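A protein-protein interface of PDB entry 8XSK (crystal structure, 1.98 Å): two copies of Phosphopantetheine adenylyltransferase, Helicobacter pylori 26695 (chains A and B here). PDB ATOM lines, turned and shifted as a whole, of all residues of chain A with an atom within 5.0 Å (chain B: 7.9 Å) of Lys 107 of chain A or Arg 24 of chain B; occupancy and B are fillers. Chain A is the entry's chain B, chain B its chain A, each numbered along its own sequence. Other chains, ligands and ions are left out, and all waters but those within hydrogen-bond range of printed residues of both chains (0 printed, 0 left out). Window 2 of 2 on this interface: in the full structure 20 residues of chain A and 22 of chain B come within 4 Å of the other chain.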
ATOM      1  N   MET A   1      17.590 -10.224  16.882  1.00  0.00           N
ATOM      2  CA  MET A   1      18.281 -10.656  15.611  1.00  0.00           C
ATOM      3  C   MET A   1      19.800 -10.532  15.771  1.00  0.00           C
ATOM      4  O   MET A   1      20.511 -11.490  15.456  1.00  0.00           O
ATOM      5  CB  MET A   1      17.845  -9.803  14.415  1.00  0.00           C
ATOM      6  CG  MET A   1      18.374 -10.324  13.088  1.00  0.00           C
ATOM      7  SD  MET A   1      18.139  -9.179  11.699  1.00  0.00           S
ATOM      8  CE  MET A   1      17.966 -10.328  10.329  1.00  0.00           C
ATOM      9  N   GLY A 103      19.879 -20.214   1.045  1.00  0.00           N
ATOM     10  CA  GLY A 103      19.235 -19.209   1.908  1.00  0.00           C
ATOM     11  C   GLY A 103      17.730 -19.423   1.991  1.00  0.00           C
ATOM     12  O   GLY A 103      17.185 -19.582   3.125  1.00  0.00           O
ATOM     13  N   TYR A 104      17.085 -19.566   0.857  1.00  0.00           N
ATOM     14  CA  TYR A 104      15.635 -19.872   0.753  1.00  0.00           C
ATOM     15  C   TYR A 104      15.308 -21.254   1.325  1.00  0.00           C
ATOM     16  O   TYR A 104      14.244 -21.348   1.971  1.00  0.00           O
ATOM     17  CB  TYR A 104      15.157 -19.708  -0.688  1.00  0.00           C
ATOM     18  CG  TYR A 104      15.246 -18.272  -1.119  1.00  0.00           C
ATOM     19  CD1 TYR A 104      14.867 -17.256  -0.252  1.00  0.00           C
ATOM     20  CD2 TYR A 104      15.738 -17.914  -2.365  1.00  0.00           C
ATOM     21  CE1 TYR A 104      14.940 -15.921  -0.616  1.00  0.00           C
ATOM     22  CE2 TYR A 104      15.817 -16.586  -2.747  1.00  0.00           C
ATOM     23  CZ  TYR A 104      15.430 -15.579  -1.861  1.00  0.00           C
ATOM     24  OH  TYR A 104      15.526 -14.243  -2.168  1.00  0.00           O
ATOM     25  N   ALA A 105      16.165 -22.270   1.129  1.00  0.00           N
ATOM     26  CA  ALA A 105      15.898 -23.628   1.665  1.00  0.00           C
ATOM     27  C   ALA A 105      15.833 -23.558   3.204  1.00  0.00           C
ATOM     28  O   ALA A 105      14.778 -23.895   3.754  1.00  0.00           O
ATOM     29  CB  ALA A 105      16.886 -24.628   1.169  1.00  0.00           C
ATOM     30  N   ASN A 106      16.875 -23.031   3.841  1.00  0.00           N
ATOM     31  CA  ASN A 106      17.017 -22.846   5.312  1.00  0.00           C
ATOM     32  C   ASN A 106      15.811 -22.077   5.889  1.00  0.00           C
ATOM     33  O   ASN A 106      15.372 -22.420   6.947  1.00  0.00           O
ATOM     34  CB  ASN A 106      18.379 -22.220   5.612  1.00  0.00           C
ATOM     35  CG  ASN A 106      19.475 -23.263   5.548  1.00  0.00           C
ATOM     36  OD1 ASN A 106      20.564 -23.021   5.049  1.00  0.00           O
ATOM     37  ND2 ASN A 106      19.198 -24.424   6.098  1.00  0.00           N
ATOM     38  N   LYS A 107      15.246 -21.104   5.180  1.00  0.00           N
ATOM     39  CA  LYS A 107      14.114 -20.271   5.688  1.00  0.00           C
ATOM     40  C   LYS A 107      12.782 -21.044   5.571  1.00  0.00           C
ATOM     41  O   LYS A 107      11.928 -20.953   6.514  1.00  0.00           O
ATOM     42  CB  LYS A 107      14.112 -18.961   4.908  1.00  0.00           C
ATOM     43  CG  LYS A 107      12.949 -18.033   5.202  1.00  0.00           C
ATOM     44  CD  LYS A 107      12.893 -17.607   6.642  1.00  0.00           C
ATOM     45  CE  LYS A 107      12.227 -16.267   6.853  1.00  0.00           C
ATOM     46  NZ  LYS A 107      12.807 -15.232   5.967  1.00  0.00           N
ATOM     47  N   SER A 108      12.591 -21.787   4.478  1.00  0.00           N
ATOM     48  CA  SER A 108      11.479 -22.769   4.329  1.00  0.00           C
ATOM     49  C   SER A 108      11.520 -23.791   5.491  1.00  0.00           C
ATOM     50  O   SER A 108      10.449 -24.153   5.960  1.00  0.00           O
ATOM     51  CB  SER A 108      11.540 -23.487   3.012  1.00  0.00           C
ATOM     52  OG  SER A 108      12.335 -24.665   3.156  1.00  0.00           O
ATOM     53  N   LEU A 109      12.705 -24.280   5.897  1.00  0.00           N
ATOM     54  CA  LEU A 109      12.834 -25.241   7.036  1.00  0.00           C
ATOM     55  C   LEU A 109      12.655 -24.474   8.361  1.00  0.00           C
ATOM     56  O   LEU A 109      12.179 -25.063   9.327  1.00  0.00           O
ATOM     57  CB  LEU A 109      14.197 -25.940   6.997  1.00  0.00           C
ATOM     58  CG  LEU A 109      14.456 -26.913   5.843  1.00  0.00           C
ATOM     59  CD1 LEU A 109      15.929 -27.290   5.785  1.00  0.00           C
ATOM     60  CD2 LEU A 109      13.629 -28.162   5.983  1.00  0.00           C
ATOM     61  N   ASN A 110      13.074 -23.211   8.455  1.00  0.00           N
ATOM     62  CA  ASN A 110      12.946 -22.466   9.739  1.00  0.00           C
ATOM     63  C   ASN A 110      12.557 -21.019   9.437  1.00  0.00           C
ATOM     64  O   ASN A 110      13.447 -20.196   9.147  1.00  0.00           O
ATOM     65  CB  ASN A 110      14.215 -22.628  10.579  1.00  0.00           C
ATOM     66  CG  ASN A 110      14.258 -21.755  11.821  1.00  0.00           C
ATOM     67  OD1 ASN A 110      13.440 -20.870  12.011  1.00  0.00           O
ATOM     68  ND2 ASN A 110      15.249 -21.966  12.663  1.00  0.00           N
ATOM     69  N   HIS A 111      11.277 -20.694   9.600  1.00  0.00           N
ATOM     70  CA  HIS A 111      10.651 -19.447   9.066  1.00  0.00           C
ATOM     71  C   HIS A 111      11.190 -18.195   9.764  1.00  0.00           C
ATOM     72  O   HIS A 111      10.947 -17.081   9.278  1.00  0.00           O
ATOM     73  CB  HIS A 111       9.126 -19.546   9.145  1.00  0.00           C
ATOM     74  CG  HIS A 111       8.597 -20.582   8.221  1.00  0.00           C
ATOM     75  ND1 HIS A 111       7.574 -21.445   8.584  1.00  0.00           N
ATOM     76  CD2 HIS A 111       8.961 -20.923   6.965  1.00  0.00           C
ATOM     77  CE1 HIS A 111       7.329 -22.271   7.592  1.00  0.00           C
ATOM     78  NE2 HIS A 111       8.153 -21.955   6.578  1.00  0.00           N
ATOM     79  N   GLU A 112      11.954 -18.377  10.826  1.00  0.00           N
ATOM     80  CA  GLU A 112      12.637 -17.265  11.527  1.00  0.00           C
ATOM     81  C   GLU A 112      14.028 -16.983  10.974  1.00  0.00           C
ATOM     82  O   GLU A 112      14.576 -15.974  11.415  1.00  0.00           O
ATOM     83  CB  GLU A 112      12.763 -17.604  12.996  1.00  0.00           C
ATOM     84  CG  GLU A 112      11.417 -17.968  13.569  1.00  0.00           C
ATOM     85  CD  GLU A 112      11.353 -17.728  15.055  1.00  0.00           C
ATOM     86  OE1 GLU A 112      12.402 -17.309  15.634  1.00  0.00           O
ATOM     87  OE2 GLU A 112      10.262 -17.949  15.620  1.00  0.00           O
ATOM     88  N   LEU A 113      14.559 -17.801  10.055  1.00  0.00           N
ATOM     89  CA  LEU A 113      16.029 -17.881   9.805  1.00  0.00           C
ATOM     90  C   LEU A 113      16.405 -17.174   8.485  1.00  0.00           C
ATOM     91  O   LEU A 113      16.125 -17.734   7.392  1.00  0.00           O
ATOM     92  CB  LEU A 113      16.452 -19.360   9.816  1.00  0.00           C
ATOM     93  CG  LEU A 113      17.962 -19.555   9.874  1.00  0.00           C
ATOM     94  CD1 LEU A 113      18.517 -18.852  11.095  1.00  0.00           C
ATOM     95  CD2 LEU A 113      18.366 -21.013   9.867  1.00  0.00           C
ATOM     96  N   GLU A 114      17.075 -16.030   8.593  1.00  0.00           N
ATOM     97  CA  GLU A 114      17.543 -15.180   7.460  1.00  0.00           C
ATOM     98  C   GLU A 114      19.033 -15.471   7.228  1.00  0.00           C
ATOM     99  O   GLU A 114      19.704 -15.879   8.191  1.00  0.00           O
ATOM    100  CB  GLU A 114      17.366 -13.698   7.807  1.00  0.00           C
ATOM    101  CG  GLU A 114      16.157 -13.399   8.699  1.00  0.00           C
ATOM    102  CD  GLU A 114      14.856 -12.999   8.034  1.00  0.00           C
ATOM    103  OE1 GLU A 114      14.792 -13.000   6.795  1.00  0.00           O
ATOM    104  OE2 GLU A 114      13.903 -12.652   8.766  1.00  0.00           O
ATOM    105  N   GLY B  17      10.971  -5.880  -3.097  1.00  0.00           N
ATOM    106  CA  GLY B  17      12.337  -6.401  -2.848  1.00  0.00           C
ATOM    107  C   GLY B  17      13.172  -5.492  -1.932  1.00  0.00           C
ATOM    108  O   GLY B  17      13.751  -5.994  -0.964  1.00  0.00           O
ATOM    109  N   HIS B  18      13.235  -4.192  -2.243  1.00  0.00           N
ATOM    110  CA  HIS B  18      13.867  -3.111  -1.431  1.00  0.00           C
ATOM    111  C   HIS B  18      13.303  -3.058  -0.012  1.00  0.00           C
ATOM    112  O   HIS B  18      14.134  -2.974   0.943  1.00  0.00           O
ATOM    113  CB  HIS B  18      13.678  -1.741  -2.090  1.00  0.00           C
ATOM    114  CG  HIS B  18      14.371  -1.623  -3.404  1.00  0.00           C
ATOM    115  ND1 HIS B  18      13.743  -1.112  -4.529  1.00  0.00           N
ATOM    116  CD2 HIS B  18      15.623  -1.952  -3.774  1.00  0.00           C
ATOM    117  CE1 HIS B  18      14.576  -1.136  -5.543  1.00  0.00           C
ATOM    118  NE2 HIS B  18      15.774  -1.608  -5.102  1.00  0.00           N
ATOM    119  N   ILE B  19      11.961  -3.012   0.105  1.00  0.00           N
ATOM    120  CA  ILE B  19      11.227  -3.047   1.404  1.00  0.00           C
ATOM    121  C   ILE B  19      11.640  -4.259   2.257  1.00  0.00           C
ATOM    122  O   ILE B  19      11.824  -4.028   3.463  1.00  0.00           O
ATOM    123  CB  ILE B  19       9.694  -2.959   1.181  1.00  0.00           C
ATOM    124  CG1 ILE B  19       9.292  -1.716   0.408  1.00  0.00           C
ATOM    125  CG2 ILE B  19       8.907  -2.987   2.481  1.00  0.00           C
ATOM    126  CD1 ILE B  19      10.090  -0.495   0.750  1.00  0.00           C
ATOM    127  N   ASP B  20      11.750  -5.488   1.715  1.00  0.00           N
ATOM    128  CA  ASP B  20      12.315  -6.651   2.455  1.00  0.00           C
ATOM    129  C   ASP B  20      13.709  -6.309   3.012  1.00  0.00           C
ATOM    130  O   ASP B  20      13.975  -6.667   4.166  1.00  0.00           O
ATOM    131  CB  ASP B  20      12.407  -7.927   1.605  1.00  0.00           C
ATOM    132  CG  ASP B  20      11.028  -8.406   1.204  1.00  0.00           C
ATOM    133  OD1 ASP B  20      10.044  -7.881   1.830  1.00  0.00           O
ATOM    134  OD2 ASP B  20      10.917  -9.275   0.322  1.00  0.00           O
ATOM    135  N   ILE B  21      14.566  -5.671   2.225  1.00  0.00           N
ATOM    136  CA  ILE B  21      15.981  -5.437   2.612  1.00  0.00           C
ATOM    137  C   ILE B  21      16.026  -4.369   3.721  1.00  0.00           C
ATOM    138  O   ILE B  21      16.848  -4.467   4.660  1.00  0.00           O
ATOM    139  CB  ILE B  21      16.826  -5.059   1.388  1.00  0.00           C
ATOM    140  CG1 ILE B  21      16.742  -6.055   0.231  1.00  0.00           C
ATOM    141  CG2 ILE B  21      18.251  -4.811   1.829  1.00  0.00           C
ATOM    142  CD1 ILE B  21      17.371  -7.386   0.496  1.00  0.00           C
ATOM    143  N   ILE B  22      15.184  -3.349   3.620  1.00  0.00           N
ATOM    144  CA  ILE B  22      15.049  -2.279   4.654  1.00  0.00           C
ATOM    145  C   ILE B  22      14.589  -2.914   5.980  1.00  0.00           C
ATOM    146  O   ILE B  22      15.178  -2.666   7.057  1.00  0.00           O
ATOM    147  CB  ILE B  22      14.088  -1.196   4.129  1.00  0.00           C
ATOM    148  CG1 ILE B  22      14.681  -0.526   2.899  1.00  0.00           C
ATOM    149  CG2 ILE B  22      13.745  -0.200   5.220  1.00  0.00           C
ATOM    150  CD1 ILE B  22      13.798   0.463   2.209  1.00  0.00           C
ATOM    151  N   HIS B  23      13.611  -3.783   5.883  1.00  0.00           N
ATOM    152  CA  HIS B  23      12.949  -4.379   7.056  1.00  0.00           C
ATOM    153  C   HIS B  23      13.983  -5.236   7.786  1.00  0.00           C
ATOM    154  O   HIS B  23      14.250  -4.984   8.967  1.00  0.00           O
ATOM    155  CB  HIS B  23      11.699  -5.105   6.582  1.00  0.00           C
ATOM    156  CG  HIS B  23      11.208  -6.019   7.633  1.00  0.00           C
ATOM    157  ND1 HIS B  23      11.234  -5.645   8.950  1.00  0.00           N
ATOM    158  CD2 HIS B  23      10.763  -7.289   7.580  1.00  0.00           C
ATOM    159  CE1 HIS B  23      10.795  -6.646   9.684  1.00  0.00           C
ATOM    160  NE2 HIS B  23      10.504  -7.675   8.866  1.00  0.00           N
ATOM    161  N   ARG B  24      14.645  -6.125   7.064  1.00  0.00           N
ATOM    162  CA  ARG B  24      15.646  -7.037   7.669  1.00  0.00           C
ATOM    163  C   ARG B  24      16.884  -6.262   8.114  1.00  0.00           C
ATOM    164  O   ARG B  24      17.322  -6.469   9.243  1.00  0.00           O
ATOM    165  CB  ARG B  24      16.025  -8.129   6.684  1.00  0.00           C
ATOM    166  CG  ARG B  24      14.889  -9.117   6.495  1.00  0.00           C
ATOM    167  CD  ARG B  24      15.155 -10.039   5.323  1.00  0.00           C
ATOM    168  NE  ARG B  24      14.076 -11.000   5.193  1.00  0.00           N
ATOM    169  CZ  ARG B  24      14.036 -11.998   4.311  1.00  0.00           C
ATOM    170  NH1 ARG B  24      12.999 -12.824   4.307  1.00  0.00           N
ATOM    171  NH2 ARG B  24      15.059 -12.199   3.500  1.00  0.00           N
ATOM    172  N   SER B  25      17.449  -5.412   7.277  1.00  0.00           N
ATOM    173  CA  SER B  25      18.710  -4.695   7.620  1.00  0.00           C
ATOM    174  C   SER B  25      18.462  -3.704   8.775  1.00  0.00           C
ATOM    175  O   SER B  25      19.327  -3.638   9.685  1.00  0.00           O
ATOM    176  CB  SER B  25      19.280  -4.002   6.431  1.00  0.00           C
ATOM    177  OG  SER B  25      18.476  -2.891   6.151  1.00  0.00           O
ATOM    178  N   SER B  26      17.302  -3.036   8.805  1.00  0.00           N
ATOM    179  CA  SER B  26      16.915  -2.075   9.875  1.00  0.00           C
ATOM    180  C   SER B  26      16.938  -2.770  11.245  1.00  0.00           C
ATOM    181  O   SER B  26      17.343  -2.109  12.186  1.00  0.00           O
ATOM    182  CB  SER B  26      15.599  -1.362   9.603  1.00  0.00           C
ATOM    183  OG  SER B  26      14.468  -2.186   9.809  1.00  0.00           O
ATOM    184  N   GLU B  27      16.644  -4.076  11.304  1.00  0.00           N
ATOM    185  CA  GLU B  27      16.607  -4.898  12.542  1.00  0.00           C
ATOM    186  C   GLU B  27      18.010  -5.009  13.138  1.00  0.00           C
ATOM    187  O   GLU B  27      18.124  -5.287  14.310  1.00  0.00           O
ATOM    188  CB  GLU B  27      16.104  -6.316  12.239  1.00  0.00           C
ATOM    189  CG  GLU B  27      14.590  -6.419  12.180  1.00  0.00           C
ATOM    190  CD  GLU B  27      14.013  -7.746  11.704  1.00  0.00           C
ATOM    191  OE1 GLU B  27      12.767  -7.868  11.689  1.00  0.00           O
ATOM    192  OE2 GLU B  27      14.788  -8.650  11.346  1.00  0.00           O
ATOM    193  N   LEU B  28      19.043  -4.841  12.319  1.00  0.00           N
ATOM    194  CA  LEU B  28      20.443  -5.148  12.699  1.00  0.00           C
ATOM    195  C   LEU B  28      21.217  -3.878  13.082  1.00  0.00           C
ATOM    196  O   LEU B  28      22.257  -4.005  13.702  1.00  0.00           O
ATOM    197  CB  LEU B  28      21.042  -5.865  11.491  1.00  0.00           C
ATOM    198  CG  LEU B  28      22.513  -6.206  11.590  1.00  0.00           C
ATOM    199  CD1 LEU B  28      22.739  -7.242  12.689  1.00  0.00           C
ATOM    200  CD2 LEU B  28      23.017  -6.667  10.227  1.00  0.00           C
ATOM    201  N   PHE B  29      20.774  -2.689  12.679  1.00  0.00           N
ATOM    202  CA  PHE B  29      21.438  -1.397  12.994  1.00  0.00           C
ATOM    203  C   PHE B  29      20.525  -0.568  13.898  1.00  0.00           C
ATOM    204  O   PHE B  29      19.330  -0.722  13.732  1.00  0.00           O
ATOM    205  CB  PHE B  29      21.737  -0.633  11.703  1.00  0.00           C
ATOM    206  CG  PHE B  29      22.665  -1.416  10.835  1.00  0.00           C
ATOM    207  CD1 PHE B  29      24.027  -1.363  11.064  1.00  0.00           C
ATOM    208  CD2 PHE B  29      22.176  -2.312   9.900  1.00  0.00           C
ATOM    209  CE1 PHE B  29      24.898  -2.162  10.336  1.00  0.00           C
ATOM    210  CE2 PHE B  29      23.057  -3.089   9.151  1.00  0.00           C
ATOM    211  CZ  PHE B  29      24.410  -3.017   9.373  1.00  0.00           C
ATOM    212  N   LEU B  32      19.093   3.146  10.248  1.00  0.00           N
ATOM    213  CA  LEU B  32      19.393   2.788   8.825  1.00  0.00           C
ATOM    214  C   LEU B  32      19.023   4.004   7.995  1.00  0.00           C
ATOM    215  O   LEU B  32      17.877   4.447   8.063  1.00  0.00           O
ATOM    216  CB  LEU B  32      18.627   1.524   8.405  1.00  0.00           C
ATOM    217  CG  LEU B  32      18.857   1.057   6.957  1.00  0.00           C
ATOM    218  CD1 LEU B  32      20.104   0.192   6.837  1.00  0.00           C
ATOM    219  CD2 LEU B  32      17.655   0.321   6.403  1.00  0.00           C
ATOM    220  N   PHE B  62       8.774   2.102   9.643  1.00  0.00           N
ATOM    221  CA  PHE B  62      10.084   1.717  10.248  1.00  0.00           C
ATOM    222  C   PHE B  62      10.683   2.937  10.960  1.00  0.00           C
ATOM    223  O   PHE B  62      11.158   3.894  10.282  1.00  0.00           O
ATOM    224  CB  PHE B  62      11.086   1.194   9.217  1.00  0.00           C
ATOM    225  CG  PHE B  62      10.589   0.056   8.366  1.00  0.00           C
ATOM    226  CD1 PHE B  62      10.315  -1.186   8.921  1.00  0.00           C
ATOM    227  CD2 PHE B  62      10.387   0.229   7.012  1.00  0.00           C
ATOM    228  CE1 PHE B  62       9.835  -2.227   8.140  1.00  0.00           C
ATOM    229  CE2 PHE B  62       9.916  -0.815   6.229  1.00  0.00           C
ATOM    230  CZ  PHE B  62       9.643  -2.039   6.793  1.00  0.00           C
ATOM    231  N   VAL B  87      24.701  -1.512   3.210  1.00  0.00           N
ATOM    232  CA  VAL B  87      23.725  -2.620   3.036  1.00  0.00           C
ATOM    233  C   VAL B  87      23.369  -2.707   1.551  1.00  0.00           C
ATOM    234  O   VAL B  87      22.983  -1.691   0.936  1.00  0.00           O
ATOM    235  CB  VAL B  87      22.520  -2.349   3.942  1.00  0.00           C
ATOM    236  CG1 VAL B  87      21.400  -3.367   3.769  1.00  0.00           C
ATOM    237  CG2 VAL B  87      22.991  -2.264   5.383  1.00  0.00           C
ATOM    238  N   PHE B 118      22.004  -8.716   2.038  1.00  0.00           N
ATOM    239  CA  PHE B 118      20.753  -9.312   2.546  1.00  0.00           C
ATOM    240  C   PHE B 118      20.041  -9.898   1.322  1.00  0.00           C
ATOM    241  O   PHE B 118      20.387  -9.548   0.167  1.00  0.00           O
ATOM    242  CB  PHE B 118      19.946  -8.268   3.342  1.00  0.00           C
ATOM    243  CG  PHE B 118      20.507  -7.847   4.682  1.00  0.00           C
ATOM    244  CD1 PHE B 118      21.521  -6.900   4.780  1.00  0.00           C
ATOM    245  CD2 PHE B 118      19.963  -8.329   5.869  1.00  0.00           C
ATOM    246  CE1 PHE B 118      22.007  -6.483   6.014  1.00  0.00           C
ATOM    247  CE2 PHE B 118      20.450  -7.908   7.098  1.00  0.00           C
ATOM    248  CZ  PHE B 118      21.470  -6.975   7.173  1.00  0.00           C
ATOM    249  N   MET B 119      19.068 -10.765   1.548  1.00  0.00           N
ATOM    250  CA  MET B 119      18.195 -11.310   0.467  1.00  0.00           C
ATOM    251  C   MET B 119      16.786 -10.804   0.706  1.00  0.00           C
ATOM    252  O   MET B 119      16.331 -10.791   1.866  1.00  0.00           O
ATOM    253  CB  MET B 119      18.152 -12.838   0.504  1.00  0.00           C
ATOM    254  CG  MET B 119      19.530 -13.508   0.506  1.00  0.00           C
ATOM    255  SD  MET B 119      19.309 -15.233   1.085  1.00  0.00           S
ATOM    256  CE  MET B 119      18.152 -15.841  -0.128  1.00  0.00           C
ATOM    257  N   PRO B 120      16.011 -10.479  -0.356  1.00  0.00           N
ATOM    258  CA  PRO B 120      14.561 -10.357  -0.196  1.00  0.00           C
ATOM    259  C   PRO B 120      13.918 -11.725   0.081  1.00  0.00           C
ATOM    260  O   PRO B 120      14.631 -12.756   0.131  1.00  0.00           O
ATOM    261  CB  PRO B 120      14.115  -9.838  -1.558  1.00  0.00           C
ATOM    262  CG  PRO B 120      15.121 -10.485  -2.507  1.00  0.00           C
ATOM    263  CD  PRO B 120      16.426 -10.358  -1.761  1.00  0.00           C
ATOM    264  N   THR B 121      12.605 -11.714   0.259  1.00  0.00           N
ATOM    265  CA  THR B 121      11.754 -12.892   0.459  1.00  0.00           C
ATOM    266  C   THR B 121      11.656 -13.638  -0.868  1.00  0.00           C
ATOM    267  O   THR B 121      11.917 -13.050  -1.919  1.00  0.00           O
ATOM    268  CB  THR B 121      10.397 -12.484   1.033  1.00  0.00           C
ATOM    269  OG1 THR B 121       9.812 -11.675   0.017  1.00  0.00           O
ATOM    270  CG2 THR B 121      10.467 -11.727   2.344  1.00  0.00           C
ATOM    271  N   LEU B 122      11.432 -14.950  -0.796  1.00  0.00           N
ATOM    272  CA  LEU B 122      11.445 -15.815  -1.983  1.00  0.00           C
ATOM    273  C   LEU B 122      10.488 -15.236  -3.033  1.00  0.00           C
ATOM    274  O   LEU B 122      10.887 -15.185  -4.206  1.00  0.00           O
ATOM    275  CB  LEU B 122      11.053 -17.237  -1.590  1.00  0.00           C
ATOM    276  CG  LEU B 122      11.347 -18.261  -2.684  1.00  0.00           C
ATOM    277  CD1 LEU B 122      11.435 -19.657  -2.109  1.00  0.00           C
ATOM    278  CD2 LEU B 122      10.288 -18.203  -3.773  1.00  0.00           C
ATOM    279  N   GLN B 123       9.300 -14.808  -2.590  1.00  0.00           N
ATOM    280  CA  GLN B 123       8.190 -14.294  -3.441  1.00  0.00           C
ATOM    281  C   GLN B 123       8.714 -13.121  -4.272  1.00  0.00           C
ATOM    282  O   GLN B 123       8.181 -12.913  -5.391  1.00  0.00           O
ATOM    283  CB  GLN B 123       7.010 -13.872  -2.557  1.00  0.00           C
ATOM    284  CG  GLN B 123       7.292 -12.607  -1.761  1.00  0.00           C
ATOM    285  CD  GLN B 123       6.272 -12.225  -0.721  1.00  0.00           C
ATOM    286  OE1 GLN B 123       6.621 -11.950   0.427  1.00  0.00           O
ATOM    287  NE2 GLN B 123       5.008 -12.168  -1.119  1.00  0.00           N
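The guanidinium group (NH1) of Arg 24 of chain B sits close to the side-chain amino group (NZ) of Lys 107 of chain A (2.9 Å).
The backbone carbonyl oxygen of Arg 24 of chain B sits close to the side-chain sulfur of Met 1 of chain A, 3.7 Å away.
The guanidinium group (NE) of Arg 24 of chain B lies within salt-bridge range of the side-chain carboxylate (OE1) of Glu 114 of chain A.
The side-chain hydroxyl (OH) of Tyr 104 of chain A is in hydrogen-bond range of the backbone carbonyl oxygen (O) of Pro 120 of chain B, 2.9 Å away.
OE2 of Glu 27 of chain B lies close to SD of Met 1 of chain A.
OE1 of Gln 123 of chain B sits close to OG1 of Thr 121 of chain B (3.2 Å).
The guanidinium group (NH2) of Arg 24 of chain B sits at hydrogen-bond distance from the backbone carbonyl oxygen (O) of Pro 120 of chain B (3.4 Å).
The side-chain carboxylate (OE1) of Glu 114 of chain A is in salt-bridge range of the side-chain amino group (NZ) of Lys 107 of chain A (3.1 Å).
The side-chain hydroxyl (OG1) of Thr 121 of chain B sits at hydrogen-bond distance from the side-chain carboxylate (OD2) of Asp 20 of chain B (2.7 Å).
The guanidinium group (NH2) of Arg 24 of chain B sits at hydrogen-bond distance from the backbone carbonyl oxygen (O) of Met 119 of chain B (2.5 Å).
Met 119 of chain B touches Tyr 104 of chain A.
O of Thr 121 of chain B touches OH of Tyr 104 of chain A, at 3.8 Å.
N of Leu 122 of chain B touches CE1 of Tyr 104 of chain A (3.6 Å).
Of the printed residues of chain B, Met 1 of chain A touches Arg 24 and Glu 27.
Of chain B, only Arg 24 comes within 4 Å of Lys 107 of chain A.
Ile 21 of chain B touches none of the printed residues of chain A.
Of chain A, only Met 1 (3.7 Å), Lys 107 (2.9 Å) and Glu 114 (2.7 Å) come within 4 Å of Arg 24 of chain B.
Of the printed residues of chain A, Glu 27 of chain B touches Met 1 (3.4 Å).
Of the printed residues of chain A, Met 119 of chain B touches Tyr 104.
Of the printed residues of chain A, Leu 122 of chain B touches Tyr 104.
The nearest printed residue of chain A that does not touch Thr 121 of chain B is Lys 107 of chain A (5.6 Å).
Hydrophobic or aromatic side chains of chain A within 4 Å of the printed part of chain B: Met 1 and Tyr 104.
No position is printed for both chains.
Of the 8 pairs that touch across the chains among the printed residues, none has its exchanged pair printed and touching as well.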
